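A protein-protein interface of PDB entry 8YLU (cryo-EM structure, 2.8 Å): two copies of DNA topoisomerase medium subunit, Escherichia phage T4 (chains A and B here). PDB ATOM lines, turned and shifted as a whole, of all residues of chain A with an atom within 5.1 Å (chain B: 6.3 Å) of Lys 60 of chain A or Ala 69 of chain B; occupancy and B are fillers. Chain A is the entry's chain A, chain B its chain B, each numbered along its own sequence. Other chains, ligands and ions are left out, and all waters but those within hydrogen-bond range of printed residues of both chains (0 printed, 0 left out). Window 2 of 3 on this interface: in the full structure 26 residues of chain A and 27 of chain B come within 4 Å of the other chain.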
ATOM      1  N   PHE A  58       7.343 -30.333  10.728  1.00  0.00           N
ATOM      2  CA  PHE A  58       6.006 -30.863  10.509  1.00  0.00           C
ATOM      3  C   PHE A  58       5.502 -30.416   9.145  1.00  0.00           C
ATOM      4  O   PHE A  58       5.536 -29.223   8.824  1.00  0.00           O
ATOM      5  CB  PHE A  58       5.049 -30.395  11.603  1.00  0.00           C
ATOM      6  CG  PHE A  58       5.075 -31.245  12.837  1.00  0.00           C
ATOM      7  CD1 PHE A  58       4.664 -32.562  12.794  1.00  0.00           C
ATOM      8  CD2 PHE A  58       5.507 -30.723  14.042  1.00  0.00           C
ATOM      9  CE1 PHE A  58       4.685 -33.344  13.927  1.00  0.00           C
ATOM     10  CE2 PHE A  58       5.530 -31.500  15.178  1.00  0.00           C
ATOM     11  CZ  PHE A  58       5.118 -32.812  15.120  1.00  0.00           C
ATOM     12  N   HIS A  59       5.037 -31.371   8.349  1.00  0.00           N
ATOM     13  CA  HIS A  59       4.553 -31.112   7.002  1.00  0.00           C
ATOM     14  C   HIS A  59       3.063 -31.401   6.926  1.00  0.00           C
ATOM     15  O   HIS A  59       2.588 -32.400   7.473  1.00  0.00           O
ATOM     16  CB  HIS A  59       5.304 -31.964   5.981  1.00  0.00           C
ATOM     17  CG  HIS A  59       6.792 -31.901   6.125  1.00  0.00           C
ATOM     18  ND1 HIS A  59       7.510 -32.842   6.828  1.00  0.00           N
ATOM     19  CD2 HIS A  59       7.696 -31.006   5.661  1.00  0.00           C
ATOM     20  CE1 HIS A  59       8.794 -32.532   6.789  1.00  0.00           C
ATOM     21  NE2 HIS A  59       8.933 -31.423   6.086  1.00  0.00           N
ATOM     22  N   LYS A  60       2.330 -30.522   6.246  1.00  0.00           N
ATOM     23  CA  LYS A  60       0.888 -30.679   6.133  1.00  0.00           C
ATOM     24  C   LYS A  60       0.547 -31.987   5.432  1.00  0.00           C
ATOM     25  O   LYS A  60       1.245 -32.417   4.512  1.00  0.00           O
ATOM     26  CB  LYS A  60       0.288 -29.498   5.372  1.00  0.00           C
ATOM     27  CG  LYS A  60      -1.134 -29.165   5.769  1.00  0.00           C
ATOM     28  CD  LYS A  60      -1.660 -27.989   4.972  1.00  0.00           C
ATOM     29  CE  LYS A  60      -1.616 -26.713   5.786  1.00  0.00           C
ATOM     30  NZ  LYS A  60      -2.275 -26.884   7.101  1.00  0.00           N
ATOM     31  N   LEU A  61      -0.531 -32.631   5.888  1.00  0.00           N
ATOM     32  CA  LEU A  61      -0.910 -33.920   5.320  1.00  0.00           C
ATOM     33  C   LEU A  61      -1.280 -33.800   3.850  1.00  0.00           C
ATOM     34  O   LEU A  61      -1.097 -34.752   3.085  1.00  0.00           O
ATOM     35  CB  LEU A  61      -2.065 -34.526   6.114  1.00  0.00           C
ATOM     36  CG  LEU A  61      -1.701 -35.773   6.918  1.00  0.00           C
ATOM     37  CD1 LEU A  61      -2.841 -36.169   7.826  1.00  0.00           C
ATOM     38  CD2 LEU A  61      -1.336 -36.917   5.990  1.00  0.00           C
ATOM     39  N   ALA A  62      -1.799 -32.642   3.435  1.00  0.00           N
ATOM     40  CA  ALA A  62      -2.016 -32.401   2.014  1.00  0.00           C
ATOM     41  C   ALA A  62      -0.699 -32.422   1.251  1.00  0.00           C
ATOM     42  O   ALA A  62      -0.621 -32.969   0.146  1.00  0.00           O
ATOM     43  CB  ALA A  62      -2.736 -31.070   1.811  1.00  0.00           C
ATOM     44  N   SER A  63       0.352 -31.840   1.835  1.00  0.00           N
ATOM     45  CA  SER A  63       1.662 -31.845   1.192  1.00  0.00           C
ATOM     46  C   SER A  63       2.219 -33.258   1.076  1.00  0.00           C
ATOM     47  O   SER A  63       2.845 -33.604   0.068  1.00  0.00           O
ATOM     48  CB  SER A  63       2.627 -30.950   1.967  1.00  0.00           C
ATOM     49  OG  SER A  63       3.963 -31.155   1.547  1.00  0.00           O
ATOM     50  N   ILE A  64       2.017 -34.084   2.104  1.00  0.00           N
ATOM     51  CA  ILE A  64       2.489 -35.463   2.051  1.00  0.00           C
ATOM     52  C   ILE A  64       1.703 -36.260   1.018  1.00  0.00           C
ATOM     53  O   ILE A  64       2.271 -37.065   0.272  1.00  0.00           O
ATOM     54  CB  ILE A  64       2.406 -36.111   3.445  1.00  0.00           C
ATOM     55  CG1 ILE A  64       3.234 -35.317   4.453  1.00  0.00           C
ATOM     56  CG2 ILE A  64       2.881 -37.550   3.393  1.00  0.00           C
ATOM     57  CD1 ILE A  64       2.834 -35.555   5.884  1.00  0.00           C
ATOM     58  N   SER A 115      -7.514 -32.612   6.243  1.00  0.00           N
ATOM     59  CA  SER A 115      -6.077 -32.576   6.008  1.00  0.00           C
ATOM     60  C   SER A 115      -5.545 -31.166   5.788  1.00  0.00           C
ATOM     61  O   SER A 115      -4.324 -30.977   5.800  1.00  0.00           O
ATOM     62  CB  SER A 115      -5.721 -33.458   4.813  1.00  0.00           C
ATOM     63  OG  SER A 115      -6.607 -33.228   3.734  1.00  0.00           O
ATOM     64  N   ARG A 116      -6.418 -30.180   5.586  1.00  0.00           N
ATOM     65  CA  ARG A 116      -5.984 -28.793   5.494  1.00  0.00           C
ATOM     66  C   ARG A 116      -5.569 -28.219   6.840  1.00  0.00           C
ATOM     67  O   ARG A 116      -5.022 -27.113   6.879  1.00  0.00           O
ATOM     68  CB  ARG A 116      -7.097 -27.935   4.893  1.00  0.00           C
ATOM     69  CG  ARG A 116      -8.416 -28.043   5.626  1.00  0.00           C
ATOM     70  CD  ARG A 116      -9.533 -27.342   4.882  1.00  0.00           C
ATOM     71  NE  ARG A 116     -10.734 -28.165   4.826  1.00  0.00           N
ATOM     72  CZ  ARG A 116     -11.817 -27.959   5.561  1.00  0.00           C
ATOM     73  NH1 ARG A 116     -11.890 -26.958   6.420  1.00  0.00           N
ATOM     74  NH2 ARG A 116     -12.853 -28.782   5.436  1.00  0.00           N
ATOM     75  N   TYR A 117      -5.813 -28.936   7.936  1.00  0.00           N
ATOM     76  CA  TYR A 117      -5.525 -28.455   9.281  1.00  0.00           C
ATOM     77  C   TYR A 117      -4.305 -29.111   9.906  1.00  0.00           C
ATOM     78  O   TYR A 117      -3.550 -28.447  10.620  1.00  0.00           O
ATOM     79  CB  TYR A 117      -6.717 -28.709  10.204  1.00  0.00           C
ATOM     80  CG  TYR A 117      -7.987 -27.996   9.832  1.00  0.00           C
ATOM     81  CD1 TYR A 117      -8.075 -26.614   9.890  1.00  0.00           C
ATOM     82  CD2 TYR A 117      -9.108 -28.710   9.448  1.00  0.00           C
ATOM     83  CE1 TYR A 117      -9.243 -25.966   9.562  1.00  0.00           C
ATOM     84  CE2 TYR A 117     -10.276 -28.072   9.120  1.00  0.00           C
ATOM     85  CZ  TYR A 117     -10.339 -26.702   9.180  1.00  0.00           C
ATOM     86  OH  TYR A 117     -11.510 -26.071   8.853  1.00  0.00           O
ATOM     87  N   ILE A 118      -4.102 -30.399   9.659  1.00  0.00           N
ATOM     88  CA  ILE A 118      -3.199 -31.216  10.456  1.00  0.00           C
ATOM     89  C   ILE A 118      -1.909 -31.472   9.690  1.00  0.00           C
ATOM     90  O   ILE A 118      -1.893 -31.556   8.456  1.00  0.00           O
ATOM     91  CB  ILE A 118      -3.881 -32.539  10.863  1.00  0.00           C
ATOM     92  CG1 ILE A 118      -4.396 -33.280   9.629  1.00  0.00           C
ATOM     93  CG2 ILE A 118      -5.027 -32.268  11.819  1.00  0.00           C
ATOM     94  CD1 ILE A 118      -5.250 -34.480   9.957  1.00  0.00           C
ATOM     95  N   PHE A 119      -0.818 -31.595  10.442  1.00  0.00           N
ATOM     96  CA  PHE A 119       0.514 -31.830   9.907  1.00  0.00           C
ATOM     97  C   PHE A 119       1.025 -33.174  10.408  1.00  0.00           C
ATOM     98  O   PHE A 119       0.525 -33.716  11.392  1.00  0.00           O
ATOM     99  CB  PHE A 119       1.493 -30.722  10.321  1.00  0.00           C
ATOM    100  CG  PHE A 119       1.007 -29.331  10.023  1.00  0.00           C
ATOM    101  CD1 PHE A 119       0.057 -28.724  10.825  1.00  0.00           C
ATOM    102  CD2 PHE A 119       1.514 -28.625   8.948  1.00  0.00           C
ATOM    103  CE1 PHE A 119      -0.387 -27.451  10.550  1.00  0.00           C
ATOM    104  CE2 PHE A 119       1.072 -27.350   8.673  1.00  0.00           C
ATOM    105  CZ  PHE A 119       0.121 -26.764   9.475  1.00  0.00           C
ATOM    106  N   ALA A 120       2.048 -33.699   9.738  1.00  0.00           N
ATOM    107  CA  ALA A 120       2.618 -34.976  10.141  1.00  0.00           C
ATOM    108  C   ALA A 120       4.103 -35.005   9.817  1.00  0.00           C
ATOM    109  O   ALA A 120       4.593 -34.260   8.966  1.00  0.00           O
ATOM    110  CB  ALA A 120       1.903 -36.149   9.463  1.00  0.00           C
ATOM    111  N   ALA B  65      -0.664 -28.218  -5.639  1.00  0.00           N
ATOM    112  CA  ALA B  65      -1.435 -27.580  -4.580  1.00  0.00           C
ATOM    113  C   ALA B  65      -1.006 -28.020  -3.187  1.00  0.00           C
ATOM    114  O   ALA B  65      -1.282 -27.305  -2.219  1.00  0.00           O
ATOM    115  CB  ALA B  65      -2.921 -27.859  -4.775  1.00  0.00           C
ATOM    116  N   GLY B  66      -0.351 -29.174  -3.055  1.00  0.00           N
ATOM    117  CA  GLY B  66       0.038 -29.640  -1.734  1.00  0.00           C
ATOM    118  C   GLY B  66       1.087 -28.766  -1.078  1.00  0.00           C
ATOM    119  O   GLY B  66       0.993 -28.457   0.114  1.00  0.00           O
ATOM    120  N   GLY B  67       2.094 -28.352  -1.837  1.00  0.00           N
ATOM    121  CA  GLY B  67       3.209 -27.615  -1.288  1.00  0.00           C
ATOM    122  C   GLY B  67       3.052 -26.117  -1.193  1.00  0.00           C
ATOM    123  O   GLY B  67       3.987 -25.445  -0.749  1.00  0.00           O
ATOM    124  N   VAL B  68       1.908 -25.557  -1.595  1.00  0.00           N
ATOM    125  CA  VAL B  68       1.744 -24.110  -1.523  1.00  0.00           C
ATOM    126  C   VAL B  68       1.617 -23.626  -0.086  1.00  0.00           C
ATOM    127  O   VAL B  68       1.923 -22.463   0.197  1.00  0.00           O
ATOM    128  CB  VAL B  68       0.532 -23.646  -2.355  1.00  0.00           C
ATOM    129  CG1 VAL B  68       0.690 -24.068  -3.804  1.00  0.00           C
ATOM    130  CG2 VAL B  68      -0.757 -24.184  -1.772  1.00  0.00           C
ATOM    131  N   ALA B  69       1.178 -24.488   0.834  1.00  0.00           N
ATOM    132  CA  ALA B  69       1.087 -24.087   2.234  1.00  0.00           C
ATOM    133  C   ALA B  69       2.462 -23.836   2.835  1.00  0.00           C
ATOM    134  O   ALA B  69       2.603 -22.995   3.729  1.00  0.00           O
ATOM    135  CB  ALA B  69       0.339 -25.147   3.038  1.00  0.00           C
ATOM    136  N   ASP B  70       3.481 -24.557   2.365  1.00  0.00           N
ATOM    137  CA  ASP B  70       4.843 -24.311   2.826  1.00  0.00           C
ATOM    138  C   ASP B  70       5.369 -22.972   2.331  1.00  0.00           C
ATOM    139  O   ASP B  70       6.242 -22.376   2.973  1.00  0.00           O
ATOM    140  CB  ASP B  70       5.759 -25.445   2.369  1.00  0.00           C
ATOM    141  CG  ASP B  70       6.987 -25.586   3.241  1.00  0.00           C
ATOM    142  OD1 ASP B  70       6.930 -25.181   4.420  1.00  0.00           O
ATOM    143  OD2 ASP B  70       8.010 -26.104   2.748  1.00  0.00           O
ATOM    144  N   LEU B  71       4.860 -22.486   1.199  1.00  0.00           N
ATOM    145  CA  LEU B  71       5.280 -21.201   0.658  1.00  0.00           C
ATOM    146  C   LEU B  71       4.595 -20.020   1.328  1.00  0.00           C
ATOM    147  O   LEU B  71       4.964 -18.875   1.051  1.00  0.00           O
ATOM    148  CB  LEU B  71       5.012 -21.147  -0.848  1.00  0.00           C
ATOM    149  CG  LEU B  71       5.537 -22.292  -1.708  1.00  0.00           C
ATOM    150  CD1 LEU B  71       4.953 -22.199  -3.099  1.00  0.00           C
ATOM    151  CD2 LEU B  71       7.050 -22.274  -1.765  1.00  0.00           C
ATOM    152  N   GLY B  72       3.610 -20.262   2.187  1.00  0.00           N
ATOM    153  CA  GLY B  72       2.944 -19.180   2.885  1.00  0.00           C
ATOM    154  C   GLY B  72       1.473 -19.050   2.554  1.00  0.00           C
ATOM    155  O   GLY B  72       0.873 -17.999   2.789  1.00  0.00           O
ATOM    156  N   TYR B  73       0.883 -20.107   2.003  1.00  0.00           N
ATOM    157  CA  TYR B  73      -0.543 -20.113   1.709  1.00  0.00           C
ATOM    158  C   TYR B  73      -1.321 -20.530   2.949  1.00  0.00           C
ATOM    159  O   TYR B  73      -1.026 -21.562   3.561  1.00  0.00           O
ATOM    160  CB  TYR B  73      -0.846 -21.055   0.546  1.00  0.00           C
ATOM    161  CG  TYR B  73      -2.232 -20.895  -0.030  1.00  0.00           C
ATOM    162  CD1 TYR B  73      -2.722 -19.645  -0.380  1.00  0.00           C
ATOM    163  CD2 TYR B  73      -3.053 -21.996  -0.225  1.00  0.00           C
ATOM    164  CE1 TYR B  73      -3.987 -19.497  -0.906  1.00  0.00           C
ATOM    165  CE2 TYR B  73      -4.317 -21.856  -0.750  1.00  0.00           C
ATOM    166  CZ  TYR B  73      -4.780 -20.606  -1.088  1.00  0.00           C
ATOM    167  OH  TYR B  73      -6.042 -20.470  -1.611  1.00  0.00           O
ATOM    168  N   HIS B  74      -2.319 -19.731   3.317  1.00  0.00           N
ATOM    169  CA  HIS B  74      -3.018 -19.891   4.584  1.00  0.00           C
ATOM    170  C   HIS B  74      -4.449 -20.383   4.409  1.00  0.00           C
ATOM    171  O   HIS B  74      -5.283 -20.171   5.294  1.00  0.00           O
ATOM    172  CB  HIS B  74      -3.004 -18.571   5.352  1.00  0.00           C
ATOM    173  CG  HIS B  74      -1.644 -18.167   5.827  1.00  0.00           C
ATOM    174  ND1 HIS B  74      -1.311 -16.860   6.103  1.00  0.00           N
ATOM    175  CD2 HIS B  74      -0.533 -18.899   6.074  1.00  0.00           C
ATOM    176  CE1 HIS B  74      -0.052 -16.804   6.501  1.00  0.00           C
ATOM    177  NE2 HIS B  74       0.443 -18.028   6.493  1.00  0.00           N
ATOM    178  N   HIS B  75      -4.751 -21.041   3.295  1.00  0.00           N
ATOM    179  CA  HIS B  75      -6.109 -21.458   2.987  1.00  0.00           C
ATOM    180  C   HIS B  75      -6.113 -22.913   2.542  1.00  0.00           C
ATOM    181  O   HIS B  75      -5.066 -23.543   2.381  1.00  0.00           O
ATOM    182  CB  HIS B  75      -6.731 -20.562   1.913  1.00  0.00           C
ATOM    183  CG  HIS B  75      -6.722 -19.110   2.267  1.00  0.00           C
ATOM    184  ND1 HIS B  75      -7.428 -18.599   3.334  1.00  0.00           N
ATOM    185  CD2 HIS B  75      -6.080 -18.060   1.704  1.00  0.00           C
ATOM    186  CE1 HIS B  75      -7.228 -17.297   3.408  1.00  0.00           C
ATOM    187  NE2 HIS B  75      -6.414 -16.943   2.430  1.00  0.00           N
ATOM    188  N   GLU B  77      -6.371 -26.237   0.313  1.00  0.00           N
ATOM    189  CA  GLU B  77      -5.722 -26.543  -0.954  1.00  0.00           C
ATOM    190  C   GLU B  77      -6.704 -26.690  -2.107  1.00  0.00           C
ATOM    191  O   GLU B  77      -6.273 -26.680  -3.263  1.00  0.00           O
ATOM    192  CB  GLU B  77      -4.887 -27.819  -0.817  1.00  0.00           C
ATOM    193  CG  GLU B  77      -3.605 -27.638  -0.013  1.00  0.00           C
ATOM    194  CD  GLU B  77      -3.855 -27.500   1.479  1.00  0.00           C
ATOM    195  OE1 GLU B  77      -4.860 -28.055   1.971  1.00  0.00           O
ATOM    196  OE2 GLU B  77      -3.047 -26.838   2.161  1.00  0.00           O
ATOM    197  N   GLU B 143       7.465 -15.436   5.932  1.00  0.00           N
ATOM    198  CA  GLU B 143       6.872 -16.708   5.546  1.00  0.00           C
ATOM    199  C   GLU B 143       6.310 -16.697   4.131  1.00  0.00           C
ATOM    200  O   GLU B 143       5.891 -17.750   3.641  1.00  0.00           O
ATOM    201  CB  GLU B 143       5.769 -17.091   6.535  1.00  0.00           C
ATOM    202  CG  GLU B 143       6.276 -17.426   7.927  1.00  0.00           C
ATOM    203  CD  GLU B 143       6.534 -16.191   8.765  1.00  0.00           C
ATOM    204  OE1 GLU B 143       5.921 -15.143   8.476  1.00  0.00           O
ATOM    205  OE2 GLU B 143       7.346 -16.267   9.710  1.00  0.00           O
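Of the 13 printed residues of chain B, 3 touch a printed residue of chain A. Hydrophobic or aromatic side chains of chain B that line the printed part of chain A: Ala 69. Among the printed residues, no Asp or Glu carboxylate lies within 4 Å of a Lys or Arg side-chain nitrogen of the other chain.
Lys 60 of chain A touches just these residues of chain B: Ala 69 (3.7 Å) and Glu 77 (3.3 Å). Of chain A, only Lys 60 (3.7 Å) comes within 4 Å of Ala 69 of chain B. Of the printed residues of chain B, Ala 62 of chain A touches Gly 66 (3.9 Å) and Glu 77 (3.7 Å). Of the printed residues of chain B, Ser 63 of chain A touches Gly 66. Of the printed residues of chain B, Arg 116 of chain A touches Glu 77. Printed residues of chain A within 4 Å of Gly 66 of chain B: Ala 62 and Ser 63. Tyr 73 of chain B touches none of the printed residues of chain A. Ser 115 of chain A touches none of the printed residues of chain B. The nearest residue of chain B that does not touch Lys 60 of chain A is Gly 66 of chain B (5.4 Å). The nearest printed residue of chain B that does not touch Ala 62 of chain A is Ala 65 of chain B (5.7 Å).
No position is printed for both chains. Of the 6 pairs that touch across the chains among the printed residues, none has its exchanged pair printed and touching as well.
Among the printed residues, pairs that only touch across the chains: Lys 60 of chain A with Glu 77 of chain B, Ser 63 of chain A with Gly 66 of chain B, Arg 116 of chain A with Glu 77 of chain B, Ala 62 of chain A with Glu 77 of chain B, Lys 60 of chain A with Ala 69 of chain B and Ala 62 of chain A with Gly 66 of chain B.
The side-chain hydroxyl (OH) of Tyr 117 of chain A is in hydrogen-bond range of the guanidinium group (NH1) of Arg 116 of chain A (2.6 Å). The side-chain amino group of Lys 60 of chain A sits at hydrogen-bond distance from the backbone carbonyl oxygen of Arg 116 of chain A (2.8 Å).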
